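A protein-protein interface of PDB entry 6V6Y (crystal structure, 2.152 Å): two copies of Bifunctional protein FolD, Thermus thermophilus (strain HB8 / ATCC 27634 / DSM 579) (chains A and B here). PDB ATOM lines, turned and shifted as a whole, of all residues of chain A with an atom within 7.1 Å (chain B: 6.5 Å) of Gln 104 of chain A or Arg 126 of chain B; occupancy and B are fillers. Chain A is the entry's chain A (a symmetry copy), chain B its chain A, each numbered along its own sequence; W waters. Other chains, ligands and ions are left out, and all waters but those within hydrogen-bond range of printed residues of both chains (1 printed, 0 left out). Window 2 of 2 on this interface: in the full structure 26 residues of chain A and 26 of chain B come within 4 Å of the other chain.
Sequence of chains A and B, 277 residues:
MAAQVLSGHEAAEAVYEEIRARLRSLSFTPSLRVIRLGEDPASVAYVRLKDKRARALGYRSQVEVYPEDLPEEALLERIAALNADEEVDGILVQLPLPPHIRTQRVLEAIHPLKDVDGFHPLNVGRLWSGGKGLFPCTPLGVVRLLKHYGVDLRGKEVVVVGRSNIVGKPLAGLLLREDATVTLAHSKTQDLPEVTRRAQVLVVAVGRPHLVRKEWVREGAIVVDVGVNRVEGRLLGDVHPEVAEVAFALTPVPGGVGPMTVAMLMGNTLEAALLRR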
ATOM      1  N   LEU A  97      13.373  39.854  24.361  1.00  0.00           N
ATOM      2  CA  LEU A  97      11.961  39.924  24.648  1.00  0.00           C
ATOM      3  C   LEU A  97      11.727  40.881  25.811  1.00  0.00           C
ATOM      4  O   LEU A  97      12.634  41.132  26.606  1.00  0.00           O
ATOM      5  CB  LEU A  97      11.430  38.526  24.957  1.00  0.00           C
ATOM      6  CG  LEU A  97      11.209  37.744  23.662  1.00  0.00           C
ATOM      7  CD1 LEU A  97      11.027  36.255  23.903  1.00  0.00           C
ATOM      8  CD2 LEU A  97       9.994  38.325  22.966  1.00  0.00           C
ATOM      9  N   ILE A 101       8.144  38.578  29.953  1.00  0.00           N
ATOM     10  CA  ILE A 101       8.100  37.342  29.178  1.00  0.00           C
ATOM     11  C   ILE A 101       9.334  36.513  29.509  1.00  0.00           C
ATOM     12  O   ILE A 101      10.455  37.035  29.514  1.00  0.00           O
ATOM     13  CB  ILE A 101       8.013  37.634  27.666  1.00  0.00           C
ATOM     14  CG1 ILE A 101       6.612  38.168  27.334  1.00  0.00           C
ATOM     15  CG2 ILE A 101       8.367  36.391  26.844  1.00  0.00           C
ATOM     16  CD1 ILE A 101       6.194  38.006  25.905  1.00  0.00           C
ATOM     17  N   ARG A 102       9.118  35.224  29.786  1.00  0.00           N
ATOM     18  CA  ARG A 102      10.195  34.294  30.114  1.00  0.00           C
ATOM     19  C   ARG A 102      10.815  33.770  28.820  1.00  0.00           C
ATOM     20  O   ARG A 102      10.243  32.898  28.153  1.00  0.00           O
ATOM     21  CB  ARG A 102       9.665  33.152  30.980  1.00  0.00           C
ATOM     22  CG  ARG A 102       9.276  33.555  32.409  1.00  0.00           C
ATOM     23  CD  ARG A 102       7.823  33.165  32.743  1.00  0.00           C
ATOM     24  NE  ARG A 102       7.589  31.731  32.560  1.00  0.00           N
ATOM     25  CZ  ARG A 102       6.480  31.089  32.923  1.00  0.00           C
ATOM     26  NH1 ARG A 102       5.478  31.755  33.492  1.00  0.00           N
ATOM     27  NH2 ARG A 102       6.372  29.780  32.711  1.00  0.00           N
ATOM     28  N   THR A 103      12.006  34.276  28.492  1.00  0.00           N
ATOM     29  CA  THR A 103      12.633  33.986  27.203  1.00  0.00           C
ATOM     30  C   THR A 103      12.859  32.489  27.003  1.00  0.00           C
ATOM     31  O   THR A 103      12.457  31.929  25.975  1.00  0.00           O
ATOM     32  CB  THR A 103      13.939  34.776  27.093  1.00  0.00           C
ATOM     33  OG1 THR A 103      13.623  36.173  27.116  1.00  0.00           O
ATOM     34  CG2 THR A 103      14.678  34.457  25.812  1.00  0.00           C
ATOM     35  N   GLN A 104      13.492  31.819  27.975  1.00  0.00           N
ATOM     36  CA  GLN A 104      13.695  30.373  27.876  1.00  0.00           C
ATOM     37  C   GLN A 104      12.379  29.657  27.573  1.00  0.00           C
ATOM     38  O   GLN A 104      12.322  28.773  26.710  1.00  0.00           O
ATOM     39  CB  GLN A 104      14.345  29.838  29.173  1.00  0.00           C
ATOM     40  CG  GLN A 104      14.000  28.369  29.550  1.00  0.00           C
ATOM     41  CD  GLN A 104      14.763  27.822  30.797  1.00  0.00           C
ATOM     42  OE1 GLN A 104      15.224  28.583  31.661  1.00  0.00           O
ATOM     43  NE2 GLN A 104      14.897  26.498  30.874  1.00  0.00           N
ATOM     44  N   ARG A 105      11.300  30.067  28.238  1.00  0.00           N
ATOM     45  CA  ARG A 105      10.011  29.426  28.023  1.00  0.00           C
ATOM     46  C   ARG A 105       9.531  29.606  26.583  1.00  0.00           C
ATOM     47  O   ARG A 105       8.978  28.675  25.986  1.00  0.00           O
ATOM     48  CB  ARG A 105       8.992  29.981  29.016  1.00  0.00           C
ATOM     49  CG  ARG A 105       7.634  29.324  28.925  1.00  0.00           C
ATOM     50  CD  ARG A 105       7.412  28.311  30.030  1.00  0.00           C
ATOM     51  NE  ARG A 105       6.004  27.905  30.133  1.00  0.00           N
ATOM     52  CZ  ARG A 105       5.387  27.061  29.298  1.00  0.00           C
ATOM     53  NH1 ARG A 105       6.041  26.521  28.273  1.00  0.00           N
ATOM     54  NH2 ARG A 105       4.103  26.756  29.487  1.00  0.00           N
ATOM     55  N   VAL A 106       9.764  30.786  25.996  1.00  0.00           N
ATOM     56  CA  VAL A 106       9.341  31.034  24.616  1.00  0.00           C
ATOM     57  C   VAL A 106      10.180  30.214  23.641  1.00  0.00           C
ATOM     58  O   VAL A 106       9.646  29.534  22.755  1.00  0.00           O
ATOM     59  CB  VAL A 106       9.421  32.537  24.297  1.00  0.00           C
ATOM     60  CG1 VAL A 106       9.405  32.776  22.781  1.00  0.00           C
ATOM     61  CG2 VAL A 106       8.292  33.276  24.992  1.00  0.00           C
ATOM     62  N   LEU A 107      11.506  30.271  23.793  1.00  0.00           N
ATOM     63  CA  LEU A 107      12.405  29.543  22.900  1.00  0.00           C
ATOM     64  C   LEU A 107      12.144  28.042  22.946  1.00  0.00           C
ATOM     65  O   LEU A 107      12.164  27.369  21.907  1.00  0.00           O
ATOM     66  CB  LEU A 107      13.866  29.855  23.266  1.00  0.00           C
ATOM     67  CG  LEU A 107      14.256  31.326  23.087  1.00  0.00           C
ATOM     68  CD1 LEU A 107      15.733  31.620  23.455  1.00  0.00           C
ATOM     69  CD2 LEU A 107      13.968  31.740  21.655  1.00  0.00           C
ATOM     70  N   GLU A 108      11.908  27.492  24.144  1.00  0.00           N
ATOM     71  CA  GLU A 108      11.611  26.063  24.260  1.00  0.00           C
ATOM     72  C   GLU A 108      10.251  25.693  23.672  1.00  0.00           C
ATOM     73  O   GLU A 108      10.010  24.507  23.403  1.00  0.00           O
ATOM     74  CB  GLU A 108      11.682  25.621  25.725  1.00  0.00           C
ATOM     75  CG  GLU A 108      13.094  25.721  26.322  1.00  0.00           C
ATOM     76  CD  GLU A 108      13.249  24.931  27.620  1.00  0.00           C
ATOM     77  OE1 GLU A 108      12.262  24.301  28.067  1.00  0.00           O
ATOM     78  OE2 GLU A 108      14.360  24.944  28.197  1.00  0.00           O
ATOM     79  N   ALA A 109       9.365  26.674  23.458  1.00  0.00           N
ATOM     80  CA  ALA A 109       8.079  26.398  22.816  1.00  0.00           C
ATOM     81  C   ALA A 109       8.202  26.187  21.314  1.00  0.00           C
ATOM     82  O   ALA A 109       7.346  25.522  20.726  1.00  0.00           O
ATOM     83  CB  ALA A 109       7.092  27.532  23.080  1.00  0.00           C
ATOM     84  N   ILE A 110       9.241  26.728  20.677  1.00  0.00           N
ATOM     85  CA  ILE A 110       9.379  26.570  19.235  1.00  0.00           C
ATOM     86  C   ILE A 110       9.708  25.123  18.925  1.00  0.00           C
ATOM     87  O   ILE A 110      10.546  24.509  19.595  1.00  0.00           O
ATOM     88  CB  ILE A 110      10.478  27.493  18.686  1.00  0.00           C
ATOM     89  CG1 ILE A 110      10.237  28.944  19.109  1.00  0.00           C
ATOM     90  CG2 ILE A 110      10.588  27.328  17.178  1.00  0.00           C
ATOM     91  CD1 ILE A 110      11.453  29.835  18.936  1.00  0.00           C
ATOM     92  N   PHE A 119      18.204  27.604  19.330  1.00  0.00           N
ATOM     93  CA  PHE A 119      18.249  27.812  20.771  1.00  0.00           C
ATOM     94  C   PHE A 119      17.496  26.742  21.558  1.00  0.00           C
ATOM     95  O   PHE A 119      17.692  26.635  22.775  1.00  0.00           O
ATOM     96  CB  PHE A 119      17.691  29.198  21.126  1.00  0.00           C
ATOM     97  CG  PHE A 119      18.526  30.341  20.601  1.00  0.00           C
ATOM     98  CD1 PHE A 119      19.893  30.182  20.393  1.00  0.00           C
ATOM     99  CD2 PHE A 119      17.948  31.581  20.328  1.00  0.00           C
ATOM    100  CE1 PHE A 119      20.673  31.232  19.903  1.00  0.00           C
ATOM    101  CE2 PHE A 119      18.712  32.636  19.847  1.00  0.00           C
ATOM    102  CZ  PHE A 119      20.075  32.462  19.624  1.00  0.00           C
ATOM    103  N   PRO A 121      16.678  23.556  23.529  1.00  0.00           N
ATOM    104  CA  PRO A 121      17.671  22.689  24.189  1.00  0.00           C
ATOM    105  C   PRO A 121      17.923  21.386  23.445  1.00  0.00           C
ATOM    106  O   PRO A 121      19.020  20.830  23.571  1.00  0.00           O
ATOM    107  CB  PRO A 121      17.065  22.448  25.580  1.00  0.00           C
ATOM    108  CG  PRO A 121      15.579  22.759  25.421  1.00  0.00           C
ATOM    109  CD  PRO A 121      15.548  23.885  24.414  1.00  0.00           C
ATOM    110  N   LEU A 122      16.974  20.904  22.635  1.00  0.00           N
ATOM    111  CA  LEU A 122      17.241  19.717  21.821  1.00  0.00           C
ATOM    112  C   LEU A 122      18.272  20.012  20.735  1.00  0.00           C
ATOM    113  O   LEU A 122      19.111  19.158  20.415  1.00  0.00           O
ATOM    114  CB  LEU A 122      15.942  19.175  21.200  1.00  0.00           C
ATOM    115  CG  LEU A 122      16.099  18.143  20.053  1.00  0.00           C
ATOM    116  CD1 LEU A 122      16.902  16.913  20.477  1.00  0.00           C
ATOM    117  CD2 LEU A 122      14.751  17.693  19.450  1.00  0.00           C
ATOM    118  N   VAL A 124      20.568  22.487  21.044  1.00  0.00           N
ATOM    119  CA  VAL A 124      21.800  22.663  21.807  1.00  0.00           C
ATOM    120  C   VAL A 124      22.387  21.306  22.164  1.00  0.00           C
ATOM    121  O   VAL A 124      23.598  21.072  22.021  1.00  0.00           O
ATOM    122  CB  VAL A 124      21.539  23.511  23.064  1.00  0.00           C
ATOM    123  CG1 VAL A 124      22.863  23.755  23.833  1.00  0.00           C
ATOM    124  CG2 VAL A 124      20.857  24.812  22.678  1.00  0.00           C
ATOM    125  N   GLY A 125      21.527  20.375  22.590  1.00  0.00           N
ATOM    126  CA  GLY A 125      22.013  19.078  23.026  1.00  0.00           C
ATOM    127  C   GLY A 125      22.543  18.243  21.879  1.00  0.00           C
ATOM    128  O   GLY A 125      23.536  17.522  22.030  1.00  0.00           O
ATOM    129  N   PRO B 121      19.618  14.500  24.853  1.00  0.00           N
ATOM    130  CA  PRO B 121      19.986  15.829  24.334  1.00  0.00           C
ATOM    131  C   PRO B 121      19.258  16.972  25.029  1.00  0.00           C
ATOM    132  O   PRO B 121      19.797  18.083  25.074  1.00  0.00           O
ATOM    133  CB  PRO B 121      19.628  15.744  22.843  1.00  0.00           C
ATOM    134  CG  PRO B 121      18.633  14.589  22.744  1.00  0.00           C
ATOM    135  CD  PRO B 121      19.103  13.612  23.796  1.00  0.00           C
ATOM    136  N   LEU B 122      18.082  16.730  25.617  1.00  0.00           N
ATOM    137  CA  LEU B 122      17.423  17.784  26.392  1.00  0.00           C
ATOM    138  C   LEU B 122      18.200  18.102  27.665  1.00  0.00           C
ATOM    139  O   LEU B 122      18.276  19.268  28.080  1.00  0.00           O
ATOM    140  CB  LEU B 122      15.973  17.392  26.726  1.00  0.00           C
ATOM    141  CG  LEU B 122      15.260  18.235  27.815  1.00  0.00           C
ATOM    142  CD1 LEU B 122      15.219  19.725  27.471  1.00  0.00           C
ATOM    143  CD2 LEU B 122      13.831  17.742  28.129  1.00  0.00           C
ATOM    144  N   ASN B 123      18.785  17.089  28.305  1.00  0.00           N
ATOM    145  CA  ASN B 123      19.621  17.382  29.462  1.00  0.00           C
ATOM    146  C   ASN B 123      20.942  18.011  29.045  1.00  0.00           C
ATOM    147  O   ASN B 123      21.441  18.922  29.719  1.00  0.00           O
ATOM    148  CB  ASN B 123      19.843  16.117  30.275  1.00  0.00           C
ATOM    149  CG  ASN B 123      18.597  15.719  31.043  1.00  0.00           C
ATOM    150  OD1 ASN B 123      17.944  16.570  31.660  1.00  0.00           O
ATOM    151  ND2 ASN B 123      18.250  14.434  31.000  1.00  0.00           N
ATOM    152  N   VAL B 124      21.531  17.541  27.942  1.00  0.00           N
ATOM    153  CA  VAL B 124      22.734  18.192  27.433  1.00  0.00           C
ATOM    154  C   VAL B 124      22.437  19.647  27.105  1.00  0.00           C
ATOM    155  O   VAL B 124      23.209  20.554  27.454  1.00  0.00           O
ATOM    156  CB  VAL B 124      23.275  17.440  26.205  1.00  0.00           C
ATOM    157  CG1 VAL B 124      24.592  18.092  25.709  1.00  0.00           C
ATOM    158  CG2 VAL B 124      23.460  15.969  26.538  1.00  0.00           C
ATOM    159  N   GLY B 125      21.286  19.895  26.470  1.00  0.00           N
ATOM    160  CA  GLY B 125      20.961  21.248  26.051  1.00  0.00           C
ATOM    161  C   GLY B 125      20.657  22.157  27.221  1.00  0.00           C
ATOM    162  O   GLY B 125      21.020  23.341  27.211  1.00  0.00           O
ATOM    163  N   ARG B 126      20.008  21.620  28.258  1.00  0.00           N
ATOM    164  CA  ARG B 126      19.799  22.413  29.465  1.00  0.00           C
ATOM    165  C   ARG B 126      21.128  22.767  30.127  1.00  0.00           C
ATOM    166  O   ARG B 126      21.290  23.868  30.666  1.00  0.00           O
ATOM    167  CB  ARG B 126      18.885  21.667  30.431  1.00  0.00           C
ATOM    168  CG  ARG B 126      17.395  21.759  30.062  1.00  0.00           C
ATOM    169  CD  ARG B 126      16.832  23.155  30.343  1.00  0.00           C
ATOM    170  NE  ARG B 126      15.419  23.261  29.973  1.00  0.00           N
ATOM    171  CZ  ARG B 126      14.408  22.877  30.755  1.00  0.00           C
ATOM    172  NH1 ARG B 126      14.654  22.366  31.958  1.00  0.00           N
ATOM    173  NH2 ARG B 126      13.147  23.003  30.338  1.00  0.00           N
ATOM    174  N   LEU B 127      22.091  21.842  30.101  1.00  0.00           N
ATOM    175  CA  LEU B 127      23.376  22.083  30.754  1.00  0.00           C
ATOM    176  C   LEU B 127      24.099  23.256  30.109  1.00  0.00           C
ATOM    177  O   LEU B 127      24.552  24.182  30.794  1.00  0.00           O
ATOM    178  CB  LEU B 127      24.249  20.830  30.669  1.00  0.00           C
ATOM    179  CG  LEU B 127      25.517  20.711  31.510  1.00  0.00           C
ATOM    180  CD1 LEU B 127      25.901  19.240  31.531  1.00  0.00           C
ATOM    181  CD2 LEU B 127      26.684  21.544  30.982  1.00  0.00           C
ATOM    182  N   TRP B 128      24.235  23.212  28.787  1.00  0.00           N
ATOM    183  CA  TRP B 128      24.952  24.250  28.065  1.00  0.00           C
ATOM    184  C   TRP B 128      24.160  25.547  27.950  1.00  0.00           C
ATOM    185  O   TRP B 128      24.770  26.601  27.769  1.00  0.00           O
ATOM    186  CB  TRP B 128      25.357  23.731  26.685  1.00  0.00           C
ATOM    187  CG  TRP B 128      26.647  22.912  26.787  1.00  0.00           C
ATOM    188  CD1 TRP B 128      26.756  21.554  26.790  1.00  0.00           C
ATOM    189  CD2 TRP B 128      27.983  23.420  26.944  1.00  0.00           C
ATOM    190  NE1 TRP B 128      28.078  21.182  26.905  1.00  0.00           N
ATOM    191  CE2 TRP B 128      28.850  22.306  27.015  1.00  0.00           C
ATOM    192  CE3 TRP B 128      28.530  24.710  27.015  1.00  0.00           C
ATOM    193  CZ2 TRP B 128      30.239  22.438  27.154  1.00  0.00           C
ATOM    194  CZ3 TRP B 128      29.911  24.848  27.155  1.00  0.00           C
ATOM    195  CH2 TRP B 128      30.749  23.716  27.223  1.00  0.00           C
ATOM    196  N   SER B 129      22.835  25.513  28.104  1.00  0.00           N
ATOM    197  CA  SER B 129      22.032  26.735  28.059  1.00  0.00           C
ATOM    198  C   SER B 129      21.869  27.420  29.411  1.00  0.00           C
ATOM    199  O   SER B 129      21.310  28.523  29.459  1.00  0.00           O
ATOM    200  CB  SER B 129      20.646  26.432  27.486  1.00  0.00           C
ATOM    201  OG  SER B 129      20.799  26.035  26.138  1.00  0.00           O
ATOM    202  N   GLY B 130      22.332  26.808  30.502  1.00  0.00           N
ATOM    203  CA  GLY B 130      22.244  27.417  31.815  1.00  0.00           C
ATOM    204  C   GLY B 130      21.011  27.074  32.626  1.00  0.00           C
ATOM    205  O   GLY B 130      20.834  27.636  33.713  1.00  0.00           O
ATOM    206  N   GLY B 131      20.156  26.174  32.147  1.00  0.00           N
ATOM    207  CA  GLY B 131      18.951  25.804  32.859  1.00  0.00           C
ATOM    208  C   GLY B 131      19.161  24.646  33.825  1.00  0.00           C
ATOM    209  O   GLY B 131      20.283  24.241  34.137  1.00  0.00           O
ATOM    210  N   LYS B 132      18.040  24.106  34.300  1.00  0.00           N
ATOM    211  CA  LYS B 132      18.022  22.990  35.239  1.00  0.00           C
ATOM    212  C   LYS B 132      17.884  21.670  34.482  1.00  0.00           C
ATOM    213  O   LYS B 132      17.242  21.606  33.426  1.00  0.00           O
ATOM    214  CB  LYS B 132      16.877  23.174  36.245  1.00  0.00           C
ATOM    215  CG  LYS B 132      15.521  22.627  35.772  1.00  0.00           C
ATOM    216  CD  LYS B 132      14.423  22.684  36.857  1.00  0.00           C
ATOM    217  CE  LYS B 132      14.752  21.828  38.084  1.00  0.00           C
ATOM    218  NZ  LYS B 132      14.154  22.394  39.345  1.00  0.00           N
ATOM    219  N   GLY B 133      18.496  20.620  35.019  1.00  0.00           N
ATOM    220  CA  GLY B 133      18.374  19.308  34.405  1.00  0.00           C
ATOM    221  C   GLY B 133      19.152  18.262  35.179  1.00  0.00           C
ATOM    222  O   GLY B 133      19.665  18.517  36.270  1.00  0.00           O
ATOM    223  N   LEU B 134      19.238  17.072  34.587  1.00  0.00           N
ATOM    224  CA  LEU B 134      20.064  15.993  35.104  1.00  0.00           C
ATOM    225  C   LEU B 134      21.322  15.894  34.244  1.00  0.00           C
ATOM    226  O   LEU B 134      21.235  15.621  33.041  1.00  0.00           O
ATOM    227  CB  LEU B 134      19.281  14.676  35.099  1.00  0.00           C
ATOM    228  CG  LEU B 134      17.990  14.598  35.938  1.00  0.00           C
ATOM    229  CD1 LEU B 134      17.161  13.367  35.594  1.00  0.00           C
ATOM    230  CD2 LEU B 134      18.331  14.592  37.404  1.00  0.00           C
ATOM    231  N   PHE B 135      22.481  16.113  34.855  1.00  0.00           N
ATOM    232  CA  PHE B 135      23.772  16.248  34.187  1.00  0.00           C
ATOM    233  C   PHE B 135      24.661  15.032  34.432  1.00  0.00           C
ATOM    234  O   PHE B 135      24.451  14.284  35.398  1.00  0.00           O
ATOM    235  CB  PHE B 135      24.470  17.511  34.692  1.00  0.00           C
ATOM    236  CG  PHE B 135      23.633  18.739  34.548  1.00  0.00           C
ATOM    237  CD1 PHE B 135      22.807  18.898  33.440  1.00  0.00           C
ATOM    238  CD2 PHE B 135      23.660  19.730  35.507  1.00  0.00           C
ATOM    239  CE1 PHE B 135      22.017  20.016  33.308  1.00  0.00           C
ATOM    240  CE2 PHE B 135      22.884  20.874  35.367  1.00  0.00           C
ATOM    241  CZ  PHE B 135      22.059  21.018  34.272  1.00  0.00           C
ATOM    242  N   ARG B 177      30.071  27.195  34.453  1.00  0.00           N
ATOM    243  CA  ARG B 177      29.106  27.676  35.430  1.00  0.00           C
ATOM    244  C   ARG B 177      29.760  28.068  36.746  1.00  0.00           C
ATOM    245  O   ARG B 177      29.171  28.845  37.503  1.00  0.00           O
ATOM    246  CB  ARG B 177      28.051  26.618  35.695  1.00  0.00           C
ATOM    247  CG  ARG B 177      27.134  26.338  34.556  1.00  0.00           C
ATOM    248  CD  ARG B 177      26.079  25.426  35.104  1.00  0.00           C
ATOM    249  NE  ARG B 177      25.109  25.067  34.108  1.00  0.00           N
ATOM    250  CZ  ARG B 177      23.870  24.687  34.390  1.00  0.00           C
ATOM    251  NH1 ARG B 177      23.477  24.615  35.644  1.00  0.00           N
ATOM    252  NH2 ARG B 177      23.027  24.384  33.411  1.00  0.00           N
HETATM  253  O   HOH W   1      15.738  25.465  33.573  1.00  0.00           O
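Of the 16 printed residues of chain B, 7 touch a printed residue of chain A. Of the 16 printed residues of chain A, 6 touch a printed residue of chain B. Hydrophobic or aromatic side chains of chain A within 4 Å of the printed part of chain B: Pro 121, Leu 122 and Val 124. Among the printed residues, 12 pairs touch across the chains. Among the printed residues, Asp or Glu carboxylates within 4 Å of a Lys or Arg side-chain nitrogen of the other chain: Glu 108 of chain A with Arg 126 of chain B (2.7 Å).
The side-chain amide nitrogen (NE2) of Gln 104 of chain A lies within hydrogen-bond range of the side-chain carboxylate (OE2) of Glu 108 of chain A. The side-chain hydroxyl (OG) of Ser 129 of chain B sits at hydrogen-bond distance from the backbone carbonyl oxygen (O) of Gly 125 of chain B, 2.9 Å away. O of Arg 126 of chain B is in hydrogen-bond range of NH2 of Arg 177 of chain B (3.3 Å). The backbone carbonyl oxygen (O) of Lys 132 of chain B is in hydrogen-bond range of the guanidinium group (NH1) of Arg 126 of chain B (3.1 Å). The backbone carbonyl oxygen (O) of Arg 126 of chain B sits at hydrogen-bond distance from the backbone NH (N) of Gly 131 of chain B (3.0 Å).
Water W1 bridges the backbone NH (N) of Lys 132 of chain B and the side-chain amide nitrogen (NE2) of Gln 104 of chain A.
Of chain B, only Arg 126 comes within 4 Å of Gln 104 of chain A. Ala 109 of chain A touches none of the printed residues of chain B. Of the printed residues of chain B, Pro 121 of chain A touches Pro 121, Leu 122 and Gly 125. Of the printed residues of chain A, Pro 121 of chain B touches Pro 121, Leu 122 and Gly 125. Printed residues of chain A within 4 Å of Leu 122 of chain B: Pro 121 (3.7 Å). Of the printed residues of chain A, Val 124 of chain B touches Gly 125 (3.8 Å). Gly 125 of chain B touches just these residues of chain A: Pro 121 (3.2 Å), Val 124 (3.8 Å) and Gly 125 (3.6 Å). Of chain A, only Gln 104 (3.4 Å) and Glu 108 (2.7 Å) come within 4 Å of Arg 126 of chain B. Of the printed residues of chain A, Trp 128 of chain B touches Val 124 (3.8 Å). The nearest residue of chain A that does not touch Arg 126 of chain B is Pro 121 of chain A (4.1 Å).
NE of Arg 126 of chain B sits close to NE2 of Gln 104 of chain A (3.4 Å). OE2 of Glu 108 of chain A lies within salt-bridge range of NE of Arg 126 of chain B. The backbone carbonyl oxygen (O) of Pro 121 of chain A sits close to the backbone carbonyl oxygen (O) of Pro 121 of chain B (3.2 Å).
Pro 121 of chain B touches its own counterpart, Pro 121 of chain A. Pro 121 of chain A touches Leu 122 of chain B, and with the chains exchanged Leu 122 of chain A touches Pro 121 of chain B. Pro 121 of chain A touches Gly 125 of chain B, and with the chains exchanged Gly 125 of chain A touches Pro 121 of chain B. Gly 125 of chain A touches its own counterpart, Gly 125 of chain B. Of the 12 pairs that touch across the chains among the printed residues, 8 have their exchanged pair printed and touching as well.
Among the printed residues, merely in contact across the chains: Pro 121 of chain A with Gly 125 of chain B (3.2 Å), Gly 125 of chain A with Pro 121 of chain B (3.2 Å), Gly 125 of chain A with Gly 125 of chain B (3.6 Å), Val 124 of chain A with Ser 129 of chain B (3.7 Å), Leu 122 of chain A with Pro 121 of chain B (3.7 Å), Pro 121 of chain A with Leu 122 of chain B (3.7 Å), Val 124 of chain A with Trp 128 of chain B (3.8 Å), Val 124 of chain A with Gly 125 of chain B (3.8 Å) and Gly 125 of chain A with Val 124 of chain B (3.8 Å).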
